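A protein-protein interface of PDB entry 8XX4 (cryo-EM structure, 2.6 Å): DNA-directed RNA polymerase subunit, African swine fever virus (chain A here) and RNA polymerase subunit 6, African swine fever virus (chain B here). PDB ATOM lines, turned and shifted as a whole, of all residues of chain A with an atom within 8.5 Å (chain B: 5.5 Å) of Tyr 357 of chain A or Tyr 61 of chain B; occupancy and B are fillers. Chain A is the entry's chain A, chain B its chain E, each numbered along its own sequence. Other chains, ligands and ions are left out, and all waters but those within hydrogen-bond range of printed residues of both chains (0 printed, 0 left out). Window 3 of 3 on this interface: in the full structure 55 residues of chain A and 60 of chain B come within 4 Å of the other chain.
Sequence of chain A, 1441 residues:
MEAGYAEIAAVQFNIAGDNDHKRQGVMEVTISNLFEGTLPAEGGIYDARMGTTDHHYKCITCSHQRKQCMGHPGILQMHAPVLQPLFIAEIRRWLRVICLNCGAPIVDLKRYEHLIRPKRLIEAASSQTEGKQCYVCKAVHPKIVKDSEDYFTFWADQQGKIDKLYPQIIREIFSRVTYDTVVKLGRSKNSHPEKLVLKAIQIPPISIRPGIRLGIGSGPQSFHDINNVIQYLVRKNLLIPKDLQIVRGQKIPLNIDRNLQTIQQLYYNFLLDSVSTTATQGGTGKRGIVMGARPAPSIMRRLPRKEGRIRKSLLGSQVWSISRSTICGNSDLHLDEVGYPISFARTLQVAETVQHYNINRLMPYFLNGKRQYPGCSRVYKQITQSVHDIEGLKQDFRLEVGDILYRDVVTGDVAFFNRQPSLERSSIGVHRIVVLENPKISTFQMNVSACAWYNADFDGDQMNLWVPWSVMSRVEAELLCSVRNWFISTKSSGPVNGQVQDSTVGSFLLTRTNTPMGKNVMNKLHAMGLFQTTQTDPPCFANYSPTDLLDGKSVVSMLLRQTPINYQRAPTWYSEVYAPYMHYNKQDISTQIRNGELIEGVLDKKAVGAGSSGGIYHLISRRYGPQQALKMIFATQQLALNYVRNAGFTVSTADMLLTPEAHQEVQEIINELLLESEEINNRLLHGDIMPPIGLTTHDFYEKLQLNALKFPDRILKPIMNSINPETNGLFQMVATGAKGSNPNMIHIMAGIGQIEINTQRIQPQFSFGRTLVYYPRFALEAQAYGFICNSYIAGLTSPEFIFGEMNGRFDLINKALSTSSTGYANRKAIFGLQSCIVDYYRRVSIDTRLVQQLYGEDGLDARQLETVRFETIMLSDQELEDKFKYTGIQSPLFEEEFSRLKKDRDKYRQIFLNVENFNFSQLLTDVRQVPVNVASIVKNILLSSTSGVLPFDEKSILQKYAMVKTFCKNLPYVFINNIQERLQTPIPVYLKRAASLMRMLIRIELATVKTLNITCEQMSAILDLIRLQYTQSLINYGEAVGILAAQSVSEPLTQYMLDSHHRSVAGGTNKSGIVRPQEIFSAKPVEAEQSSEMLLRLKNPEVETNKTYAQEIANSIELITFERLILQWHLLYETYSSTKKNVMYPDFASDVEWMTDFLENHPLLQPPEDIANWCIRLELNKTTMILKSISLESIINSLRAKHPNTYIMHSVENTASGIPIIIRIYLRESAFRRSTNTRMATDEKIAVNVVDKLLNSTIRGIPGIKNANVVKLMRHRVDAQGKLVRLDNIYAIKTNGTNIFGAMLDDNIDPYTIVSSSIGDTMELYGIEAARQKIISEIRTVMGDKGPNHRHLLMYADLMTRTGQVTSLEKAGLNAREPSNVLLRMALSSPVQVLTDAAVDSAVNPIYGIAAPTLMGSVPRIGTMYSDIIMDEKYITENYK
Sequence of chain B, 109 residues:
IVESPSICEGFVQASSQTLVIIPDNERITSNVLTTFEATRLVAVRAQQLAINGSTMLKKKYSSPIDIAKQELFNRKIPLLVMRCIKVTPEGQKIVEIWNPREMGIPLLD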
ATOM      1  N   GLU A 352     -12.907   8.820 -19.096  1.00  0.00           N
ATOM      2  CA  GLU A 352     -14.085   8.895 -18.240  1.00  0.00           C
ATOM      3  C   GLU A 352     -14.359  10.356 -17.917  1.00  0.00           C
ATOM      4  O   GLU A 352     -13.579  10.997 -17.207  1.00  0.00           O
ATOM      5  CB  GLU A 352     -13.886   8.081 -16.968  1.00  0.00           C
ATOM      6  CG  GLU A 352     -13.814   6.592 -17.204  1.00  0.00           C
ATOM      7  CD  GLU A 352     -15.032   5.872 -16.680  1.00  0.00           C
ATOM      8  OE1 GLU A 352     -16.077   6.526 -16.502  1.00  0.00           O
ATOM      9  OE2 GLU A 352     -14.947   4.650 -16.445  1.00  0.00           O
ATOM     10  N   THR A 353     -15.466  10.879 -18.438  1.00  0.00           N
ATOM     11  CA  THR A 353     -15.870  12.237 -18.113  1.00  0.00           C
ATOM     12  C   THR A 353     -16.399  12.289 -16.688  1.00  0.00           C
ATOM     13  O   THR A 353     -17.271  11.503 -16.310  1.00  0.00           O
ATOM     14  CB  THR A 353     -16.934  12.732 -19.088  1.00  0.00           C
ATOM     15  OG1 THR A 353     -16.450  12.605 -20.428  1.00  0.00           O
ATOM     16  CG2 THR A 353     -17.259  14.183 -18.815  1.00  0.00           C
ATOM     17  N   VAL A 354     -15.867  13.215 -15.900  1.00  0.00           N
ATOM     18  CA  VAL A 354     -16.222  13.313 -14.492  1.00  0.00           C
ATOM     19  C   VAL A 354     -17.577  13.993 -14.363  1.00  0.00           C
ATOM     20  O   VAL A 354     -17.786  15.093 -14.881  1.00  0.00           O
ATOM     21  CB  VAL A 354     -15.144  14.074 -13.709  1.00  0.00           C
ATOM     22  CG1 VAL A 354     -15.484  14.081 -12.241  1.00  0.00           C
ATOM     23  CG2 VAL A 354     -13.785  13.446 -13.934  1.00  0.00           C
ATOM     24  N   GLN A 355     -18.503  13.327 -13.682  1.00  0.00           N
ATOM     25  CA  GLN A 355     -19.797  13.894 -13.348  1.00  0.00           C
ATOM     26  C   GLN A 355     -20.078  13.574 -11.888  1.00  0.00           C
ATOM     27  O   GLN A 355     -19.261  12.961 -11.200  1.00  0.00           O
ATOM     28  CB  GLN A 355     -20.902  13.359 -14.267  1.00  0.00           C
ATOM     29  CG  GLN A 355     -20.721  13.707 -15.729  1.00  0.00           C
ATOM     30  CD  GLN A 355     -21.203  15.101 -16.060  1.00  0.00           C
ATOM     31  OE1 GLN A 355     -22.184  15.578 -15.497  1.00  0.00           O
ATOM     32  NE2 GLN A 355     -20.513  15.763 -16.979  1.00  0.00           N
ATOM     33  N   HIS A 356     -21.244  13.999 -11.408  1.00  0.00           N
ATOM     34  CA  HIS A 356     -21.570  13.772 -10.007  1.00  0.00           C
ATOM     35  C   HIS A 356     -21.761  12.292  -9.706  1.00  0.00           C
ATOM     36  O   HIS A 356     -21.424  11.838  -8.608  1.00  0.00           O
ATOM     37  CB  HIS A 356     -22.818  14.564  -9.620  1.00  0.00           C
ATOM     38  CG  HIS A 356     -24.027  14.229 -10.436  1.00  0.00           C
ATOM     39  ND1 HIS A 356     -24.974  13.317 -10.022  1.00  0.00           N
ATOM     40  CD2 HIS A 356     -24.447  14.688 -11.639  1.00  0.00           C
ATOM     41  CE1 HIS A 356     -25.923  13.225 -10.937  1.00  0.00           C
ATOM     42  NE2 HIS A 356     -25.627  14.047 -11.929  1.00  0.00           N
ATOM     43  N   TYR A 357     -22.286  11.523 -10.661  1.00  0.00           N
ATOM     44  CA  TYR A 357     -22.606  10.128 -10.390  1.00  0.00           C
ATOM     45  C   TYR A 357     -21.372   9.238 -10.349  1.00  0.00           C
ATOM     46  O   TYR A 357     -21.447   8.129  -9.813  1.00  0.00           O
ATOM     47  CB  TYR A 357     -23.598   9.596 -11.429  1.00  0.00           C
ATOM     48  CG  TYR A 357     -23.229   9.883 -12.867  1.00  0.00           C
ATOM     49  CD1 TYR A 357     -22.198   9.195 -13.493  1.00  0.00           C
ATOM     50  CD2 TYR A 357     -23.918  10.833 -13.602  1.00  0.00           C
ATOM     51  CE1 TYR A 357     -21.859   9.453 -14.800  1.00  0.00           C
ATOM     52  CE2 TYR A 357     -23.587  11.094 -14.914  1.00  0.00           C
ATOM     53  CZ  TYR A 357     -22.556  10.402 -15.506  1.00  0.00           C
ATOM     54  OH  TYR A 357     -22.221  10.662 -16.810  1.00  0.00           O
ATOM     55  N   ASN A 358     -20.239   9.691 -10.890  1.00  0.00           N
ATOM     56  CA  ASN A 358     -19.049   8.854 -10.967  1.00  0.00           C
ATOM     57  C   ASN A 358     -17.823   9.480 -10.314  1.00  0.00           C
ATOM     58  O   ASN A 358     -16.724   8.938 -10.457  1.00  0.00           O
ATOM     59  CB  ASN A 358     -18.731   8.508 -12.426  1.00  0.00           C
ATOM     60  CG  ASN A 358     -18.467   9.730 -13.270  1.00  0.00           C
ATOM     61  OD1 ASN A 358     -18.919  10.821 -12.949  1.00  0.00           O
ATOM     62  ND2 ASN A 358     -17.735   9.553 -14.359  1.00  0.00           N
ATOM     63  N   ILE A 359     -17.977  10.595  -9.598  1.00  0.00           N
ATOM     64  CA  ILE A 359     -16.821  11.247  -8.988  1.00  0.00           C
ATOM     65  C   ILE A 359     -16.216  10.368  -7.899  1.00  0.00           C
ATOM     66  O   ILE A 359     -14.990  10.279  -7.765  1.00  0.00           O
ATOM     67  CB  ILE A 359     -17.213  12.641  -8.458  1.00  0.00           C
ATOM     68  CG1 ILE A 359     -16.023  13.321  -7.783  1.00  0.00           C
ATOM     69  CG2 ILE A 359     -18.409  12.561  -7.525  1.00  0.00           C
ATOM     70  CD1 ILE A 359     -15.066  13.959  -8.733  1.00  0.00           C
ATOM     71  N   ASN A 360     -17.059   9.697  -7.111  1.00  0.00           N
ATOM     72  CA  ASN A 360     -16.549   8.854  -6.034  1.00  0.00           C
ATOM     73  C   ASN A 360     -15.813   7.637  -6.576  1.00  0.00           C
ATOM     74  O   ASN A 360     -14.818   7.198  -5.991  1.00  0.00           O
ATOM     75  CB  ASN A 360     -17.691   8.428  -5.116  1.00  0.00           C
ATOM     76  CG  ASN A 360     -18.432   9.608  -4.528  1.00  0.00           C
ATOM     77  OD1 ASN A 360     -18.093  10.760  -4.791  1.00  0.00           O
ATOM     78  ND2 ASN A 360     -19.455   9.329  -3.731  1.00  0.00           N
ATOM     79  N   ARG A 361     -16.295   7.067  -7.683  1.00  0.00           N
ATOM     80  CA  ARG A 361     -15.613   5.927  -8.286  1.00  0.00           C
ATOM     81  C   ARG A 361     -14.326   6.357  -8.979  1.00  0.00           C
ATOM     82  O   ARG A 361     -13.333   5.623  -8.968  1.00  0.00           O
ATOM     83  CB  ARG A 361     -16.544   5.222  -9.271  1.00  0.00           C
ATOM     84  CG  ARG A 361     -15.825   4.340 -10.273  1.00  0.00           C
ATOM     85  CD  ARG A 361     -16.788   3.508 -11.091  1.00  0.00           C
ATOM     86  NE  ARG A 361     -17.507   4.323 -12.062  1.00  0.00           N
ATOM     87  CZ  ARG A 361     -16.991   4.759 -13.203  1.00  0.00           C
ATOM     88  NH1 ARG A 361     -15.751   4.469 -13.556  1.00  0.00           N
ATOM     89  NH2 ARG A 361     -17.739   5.507 -14.008  1.00  0.00           N
ATOM     90  N   LEU A 362     -14.324   7.542  -9.588  1.00  0.00           N
ATOM     91  CA  LEU A 362     -13.142   8.036 -10.281  1.00  0.00           C
ATOM     92  C   LEU A 362     -12.097   8.596  -9.331  1.00  0.00           C
ATOM     93  O   LEU A 362     -10.952   8.797  -9.744  1.00  0.00           O
ATOM     94  CB  LEU A 362     -13.533   9.116 -11.288  1.00  0.00           C
ATOM     95  CG  LEU A 362     -14.299   8.667 -12.529  1.00  0.00           C
ATOM     96  CD1 LEU A 362     -14.484   9.843 -13.458  1.00  0.00           C
ATOM     97  CD2 LEU A 362     -13.578   7.536 -13.229  1.00  0.00           C
ATOM     98  N   VAL A 401     -16.941  18.697 -12.673  1.00  0.00           N
ATOM     99  CA  VAL A 401     -17.893  18.082 -13.589  1.00  0.00           C
ATOM    100  C   VAL A 401     -17.662  18.635 -14.987  1.00  0.00           C
ATOM    101  O   VAL A 401     -17.698  19.851 -15.210  1.00  0.00           O
ATOM    102  CB  VAL A 401     -19.336  18.314 -13.118  1.00  0.00           C
ATOM    103  CG1 VAL A 401     -19.658  17.395 -11.958  1.00  0.00           C
ATOM    104  CG2 VAL A 401     -19.546  19.758 -12.717  1.00  0.00           C
ATOM    105  N   VAL A 471     -17.343   6.805 -24.867  1.00  0.00           N
ATOM    106  CA  VAL A 471     -18.561   6.231 -24.312  1.00  0.00           C
ATOM    107  C   VAL A 471     -19.381   5.548 -25.399  1.00  0.00           C
ATOM    108  O   VAL A 471     -19.952   4.474 -25.182  1.00  0.00           O
ATOM    109  CB  VAL A 471     -19.359   7.326 -23.581  1.00  0.00           C
ATOM    110  CG1 VAL A 471     -20.827   7.090 -23.721  1.00  0.00           C
ATOM    111  CG2 VAL A 471     -18.976   7.361 -22.121  1.00  0.00           C
ATOM    112  N   ALA B  46     -25.826   7.732 -23.428  1.00  0.00           N
ATOM    113  CA  ALA B  46     -24.693   7.661 -22.516  1.00  0.00           C
ATOM    114  C   ALA B  46     -23.709   8.796 -22.759  1.00  0.00           C
ATOM    115  O   ALA B  46     -23.175   9.372 -21.807  1.00  0.00           O
ATOM    116  CB  ALA B  46     -24.011   6.305 -22.647  1.00  0.00           C
ATOM    117  N   LEU B  49     -25.283  11.808 -21.252  1.00  0.00           N
ATOM    118  CA  LEU B  49     -25.112  11.746 -19.806  1.00  0.00           C
ATOM    119  C   LEU B  49     -23.669  11.970 -19.396  1.00  0.00           C
ATOM    120  O   LEU B  49     -23.404  12.236 -18.222  1.00  0.00           O
ATOM    121  CB  LEU B  49     -25.586  10.400 -19.268  1.00  0.00           C
ATOM    122  CG  LEU B  49     -27.085  10.135 -19.260  1.00  0.00           C
ATOM    123  CD1 LEU B  49     -27.338   8.651 -19.359  1.00  0.00           C
ATOM    124  CD2 LEU B  49     -27.711  10.699 -18.008  1.00  0.00           C
ATOM    125  N   ALA B  50     -22.728  11.804 -20.320  1.00  0.00           N
ATOM    126  CA  ALA B  50     -21.350  12.178 -20.037  1.00  0.00           C
ATOM    127  C   ALA B  50     -21.160  13.688 -20.119  1.00  0.00           C
ATOM    128  O   ALA B  50     -20.376  14.257 -19.355  1.00  0.00           O
ATOM    129  CB  ALA B  50     -20.399  11.463 -20.992  1.00  0.00           C
ATOM    130  N   ASN B  52     -23.951  16.003 -20.035  1.00  0.00           N
ATOM    131  CA  ASN B  52     -24.902  16.457 -19.034  1.00  0.00           C
ATOM    132  C   ASN B  52     -24.803  15.526 -17.830  1.00  0.00           C
ATOM    133  O   ASN B  52     -23.858  14.749 -17.703  1.00  0.00           O
ATOM    134  CB  ASN B  52     -26.311  16.506 -19.628  1.00  0.00           C
ATOM    135  CG  ASN B  52     -27.264  17.365 -18.819  1.00  0.00           C
ATOM    136  OD1 ASN B  52     -27.546  17.072 -17.659  1.00  0.00           O
ATOM    137  ND2 ASN B  52     -27.770  18.426 -19.429  1.00  0.00           N
ATOM    138  N   GLY B  53     -25.756  15.622 -16.909  1.00  0.00           N
ATOM    139  CA  GLY B  53     -25.789  14.671 -15.816  1.00  0.00           C
ATOM    140  C   GLY B  53     -27.181  14.291 -15.360  1.00  0.00           C
ATOM    141  O   GLY B  53     -27.339  13.467 -14.456  1.00  0.00           O
ATOM    142  N   LEU B  57     -33.493   8.226 -13.433  1.00  0.00           N
ATOM    143  CA  LEU B  57     -33.299   6.917 -12.830  1.00  0.00           C
ATOM    144  C   LEU B  57     -33.286   7.058 -11.314  1.00  0.00           C
ATOM    145  O   LEU B  57     -32.407   7.726 -10.757  1.00  0.00           O
ATOM    146  CB  LEU B  57     -31.997   6.292 -13.320  1.00  0.00           C
ATOM    147  CG  LEU B  57     -32.029   5.549 -14.651  1.00  0.00           C
ATOM    148  CD1 LEU B  57     -30.875   4.589 -14.691  1.00  0.00           C
ATOM    149  CD2 LEU B  57     -33.341   4.814 -14.834  1.00  0.00           C
ATOM    150  N   LYS B  59     -32.733   4.577  -9.169  1.00  0.00           N
ATOM    151  CA  LYS B  59     -31.512   3.890  -8.775  1.00  0.00           C
ATOM    152  C   LYS B  59     -30.310   4.636  -9.333  1.00  0.00           C
ATOM    153  O   LYS B  59     -30.313   5.058 -10.493  1.00  0.00           O
ATOM    154  CB  LYS B  59     -31.525   2.444  -9.265  1.00  0.00           C
ATOM    155  CG  LYS B  59     -30.198   1.726  -9.094  1.00  0.00           C
ATOM    156  CD  LYS B  59     -30.391   0.241  -8.846  1.00  0.00           C
ATOM    157  CE  LYS B  59     -29.484  -0.255  -7.729  1.00  0.00           C
ATOM    158  NZ  LYS B  59     -29.935   0.197  -6.384  1.00  0.00           N
ATOM    159  N   LYS B  60     -29.287   4.813  -8.505  1.00  0.00           N
ATOM    160  CA  LYS B  60     -28.117   5.585  -8.889  1.00  0.00           C
ATOM    161  C   LYS B  60     -27.048   4.661  -9.451  1.00  0.00           C
ATOM    162  O   LYS B  60     -26.685   3.662  -8.823  1.00  0.00           O
ATOM    163  CB  LYS B  60     -27.572   6.369  -7.695  1.00  0.00           C
ATOM    164  CG  LYS B  60     -28.480   7.492  -7.218  1.00  0.00           C
ATOM    165  CD  LYS B  60     -29.196   8.169  -8.376  1.00  0.00           C
ATOM    166  CE  LYS B  60     -29.222   9.682  -8.204  1.00  0.00           C
ATOM    167  NZ  LYS B  60     -29.829  10.090  -6.908  1.00  0.00           N
ATOM    168  N   TYR B  61     -26.553   4.994 -10.639  1.00  0.00           N
ATOM    169  CA  TYR B  61     -25.495   4.245 -11.295  1.00  0.00           C
ATOM    170  C   TYR B  61     -24.282   5.142 -11.472  1.00  0.00           C
ATOM    171  O   TYR B  61     -24.416   6.347 -11.702  1.00  0.00           O
ATOM    172  CB  TYR B  61     -25.945   3.702 -12.651  1.00  0.00           C
ATOM    173  CG  TYR B  61     -27.072   2.708 -12.559  1.00  0.00           C
ATOM    174  CD1 TYR B  61     -28.390   3.125 -12.534  1.00  0.00           C
ATOM    175  CD2 TYR B  61     -26.816   1.347 -12.517  1.00  0.00           C
ATOM    176  CE1 TYR B  61     -29.418   2.220 -12.454  1.00  0.00           C
ATOM    177  CE2 TYR B  61     -27.837   0.435 -12.434  1.00  0.00           C
ATOM    178  CZ  TYR B  61     -29.136   0.875 -12.402  1.00  0.00           C
ATOM    179  OH  TYR B  61     -30.159  -0.040 -12.324  1.00  0.00           O
ATOM    180  N   SER B  62     -23.102   4.549 -11.358  1.00  0.00           N
ATOM    181  CA  SER B  62     -21.855   5.291 -11.444  1.00  0.00           C
ATOM    182  C   SER B  62     -21.269   5.308 -12.845  1.00  0.00           C
ATOM    183  O   SER B  62     -20.143   5.781 -13.024  1.00  0.00           O
ATOM    184  CB  SER B  62     -20.831   4.708 -10.474  1.00  0.00           C
ATOM    185  OG  SER B  62     -19.528   4.853 -10.999  1.00  0.00           O
ATOM    186  N   SER B  63     -21.988   4.791 -13.835  1.00  0.00           N
ATOM    187  CA  SER B  63     -21.520   4.783 -15.206  1.00  0.00           C
ATOM    188  C   SER B  63     -22.616   5.313 -16.117  1.00  0.00           C
ATOM    189  O   SER B  63     -23.784   4.944 -15.959  1.00  0.00           O
ATOM    190  CB  SER B  63     -21.117   3.368 -15.640  1.00  0.00           C
ATOM    191  OG  SER B  63     -21.149   3.233 -17.047  1.00  0.00           O
ATOM    192  N   PRO B  64     -22.279   6.193 -17.061  1.00  0.00           N
ATOM    193  CA  PRO B  64     -23.300   6.659 -18.011  1.00  0.00           C
ATOM    194  C   PRO B  64     -23.870   5.537 -18.847  1.00  0.00           C
ATOM    195  O   PRO B  64     -25.040   5.593 -19.241  1.00  0.00           O
ATOM    196  CB  PRO B  64     -22.538   7.678 -18.867  1.00  0.00           C
ATOM    197  CG  PRO B  64     -21.118   7.266 -18.764  1.00  0.00           C
ATOM    198  CD  PRO B  64     -20.942   6.715 -17.383  1.00  0.00           C
ATOM    199  N   ASP B  66     -24.434   2.404 -17.844  1.00  0.00           N
ATOM    200  CA  ASP B  66     -25.460   1.740 -17.045  1.00  0.00           C
ATOM    201  C   ASP B  66     -26.739   2.563 -16.985  1.00  0.00           C
ATOM    202  O   ASP B  66     -27.843   2.017 -17.100  1.00  0.00           O
ATOM    203  CB  ASP B  66     -24.943   1.471 -15.635  1.00  0.00           C
ATOM    204  CG  ASP B  66     -23.556   0.882 -15.630  1.00  0.00           C
ATOM    205  OD1 ASP B  66     -23.041   0.574 -16.722  1.00  0.00           O
ATOM    206  OD2 ASP B  66     -22.981   0.722 -14.533  1.00  0.00           O
ATOM    207  N   ILE B  67     -26.612   3.878 -16.805  1.00  0.00           N
ATOM    208  CA  ILE B  67     -27.791   4.737 -16.762  1.00  0.00           C
ATOM    209  C   ILE B  67     -28.544   4.670 -18.082  1.00  0.00           C
ATOM    210  O   ILE B  67     -29.771   4.561 -18.107  1.00  0.00           O
ATOM    211  CB  ILE B  67     -27.395   6.185 -16.422  1.00  0.00           C
ATOM    212  CG1 ILE B  67     -26.665   6.248 -15.087  1.00  0.00           C
ATOM    213  CG2 ILE B  67     -28.621   7.067 -16.385  1.00  0.00           C
ATOM    214  CD1 ILE B  67     -26.030   7.582 -14.820  1.00  0.00           C
ATOM    215  N   GLN B  70     -30.304   1.282 -18.522  1.00  0.00           N
ATOM    216  CA  GLN B  70     -31.503   1.181 -17.702  1.00  0.00           C
ATOM    217  C   GLN B  70     -32.604   2.100 -18.214  1.00  0.00           C
ATOM    218  O   GLN B  70     -33.785   1.753 -18.144  1.00  0.00           O
ATOM    219  CB  GLN B  70     -31.172   1.484 -16.246  1.00  0.00           C
ATOM    220  CG  GLN B  70     -30.326   0.426 -15.587  1.00  0.00           C
ATOM    221  CD  GLN B  70     -30.813  -0.972 -15.885  1.00  0.00           C
ATOM    222  OE1 GLN B  70     -31.978  -1.297 -15.666  1.00  0.00           O
ATOM    223  NE2 GLN B  70     -29.921  -1.811 -16.394  1.00  0.00           N
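Thr 353 of chain A touches Ala 50 of chain B.
CG of Gln 355 of chain A touches O of Leu 49 of chain B, at 3.9 Å.
CA of Gly 53 of chain B touches OE1 of Gln 355 of chain A (3.7 Å).
CA of Ala 50 of chain B touches OH of Tyr 357 of chain A (3.7 Å).
Tyr 61 of chain B touches Tyr 357 of chain A.
O of Tyr 357 of chain A touches CA of Ser 62 of chain B, 3.3 Å away.
Tyr 357 of chain A touches Pro 64 of chain B.
Ser 62 of chain B touches Asn 358 of chain A.
Ala 46 of chain B touches Val 471 of chain A (CB to CG1, 3.5 Å).
Pro 64 of chain B touches Val 471 of chain A (CG to CG2, 3.98 Å).
Hydrophobic or aromatic side chains of chain A that line the printed part of chain B: His 356, Tyr 357 and Val 471.
Along chain A the printed residues that touch a printed residue of chain B span positions 353 to 471.
Of the 15 printed residues of chain B, 8 touch a printed residue of chain A.
Among the printed residues, no Asp or Glu carboxylate lies within 4 Å of a Lys or Arg side-chain nitrogen of the other chain.
The side-chain amide nitrogen (NE2) of Gln 355 of chain A sits at hydrogen-bond distance from the backbone carbonyl oxygen (O) of Ala 50 of chain B (2.8 Å).
OE1 of Gln 355 of chain A lies close to O of Asn 52 of chain B, 2.9 Å away.
A ring nitrogen (NE2) of His 356 of chain A is in hydrogen-bond range of the backbone carbonyl oxygen (O) of Gly 53 of chain B (3.1 Å).
The backbone carbonyl oxygen (O) of Leu 49 of chain B is in hydrogen-bond range of the side-chain hydroxyl (OH) of Tyr 357 of chain A, at 2.4 Å.
NH2 of Arg 361 of chain A lies within hydrogen-bond range of O of Ser 62 of chain B (2.6 Å).
Glu 352 of chain A touches none of the printed residues of chain B.
Of the printed residues of chain B, Thr 353 of chain A touches Ala 50.
Tyr 357 of chain A touches five residues of chain B.
Of the printed residues of chain A, Asn 52 of chain B touches Gln 355 (2.9 Å).
Tyr 61 of chain B touches just one residue of chain A: Tyr 357.
Ser 62 of chain B touches three residues of chain A.
Of the printed residues of chain A, Pro 64 of chain B touches Tyr 357 and Val 471.
Ile 67 of chain B touches none of the printed residues of chain A.
The nearest printed residue of chain B that does not touch Val 471 of chain A is Ala 50 of chain B (4.5 Å).
The guanidinium group of Arg 361 of chain A lies within salt-bridge range of the side-chain carboxylate of Glu 352 of chain A, 3.0 Å away.
The backbone carbonyl oxygen (O) of Thr 353 of chain A is in hydrogen-bond range of the side-chain amide nitrogen (ND2) of Asn 358 of chain A (2.8 Å).
The backbone NH of Gln 355 of chain A sits at hydrogen-bond distance from the side-chain amide oxygen of Asn 358 of chain A, 2.6 Å away.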
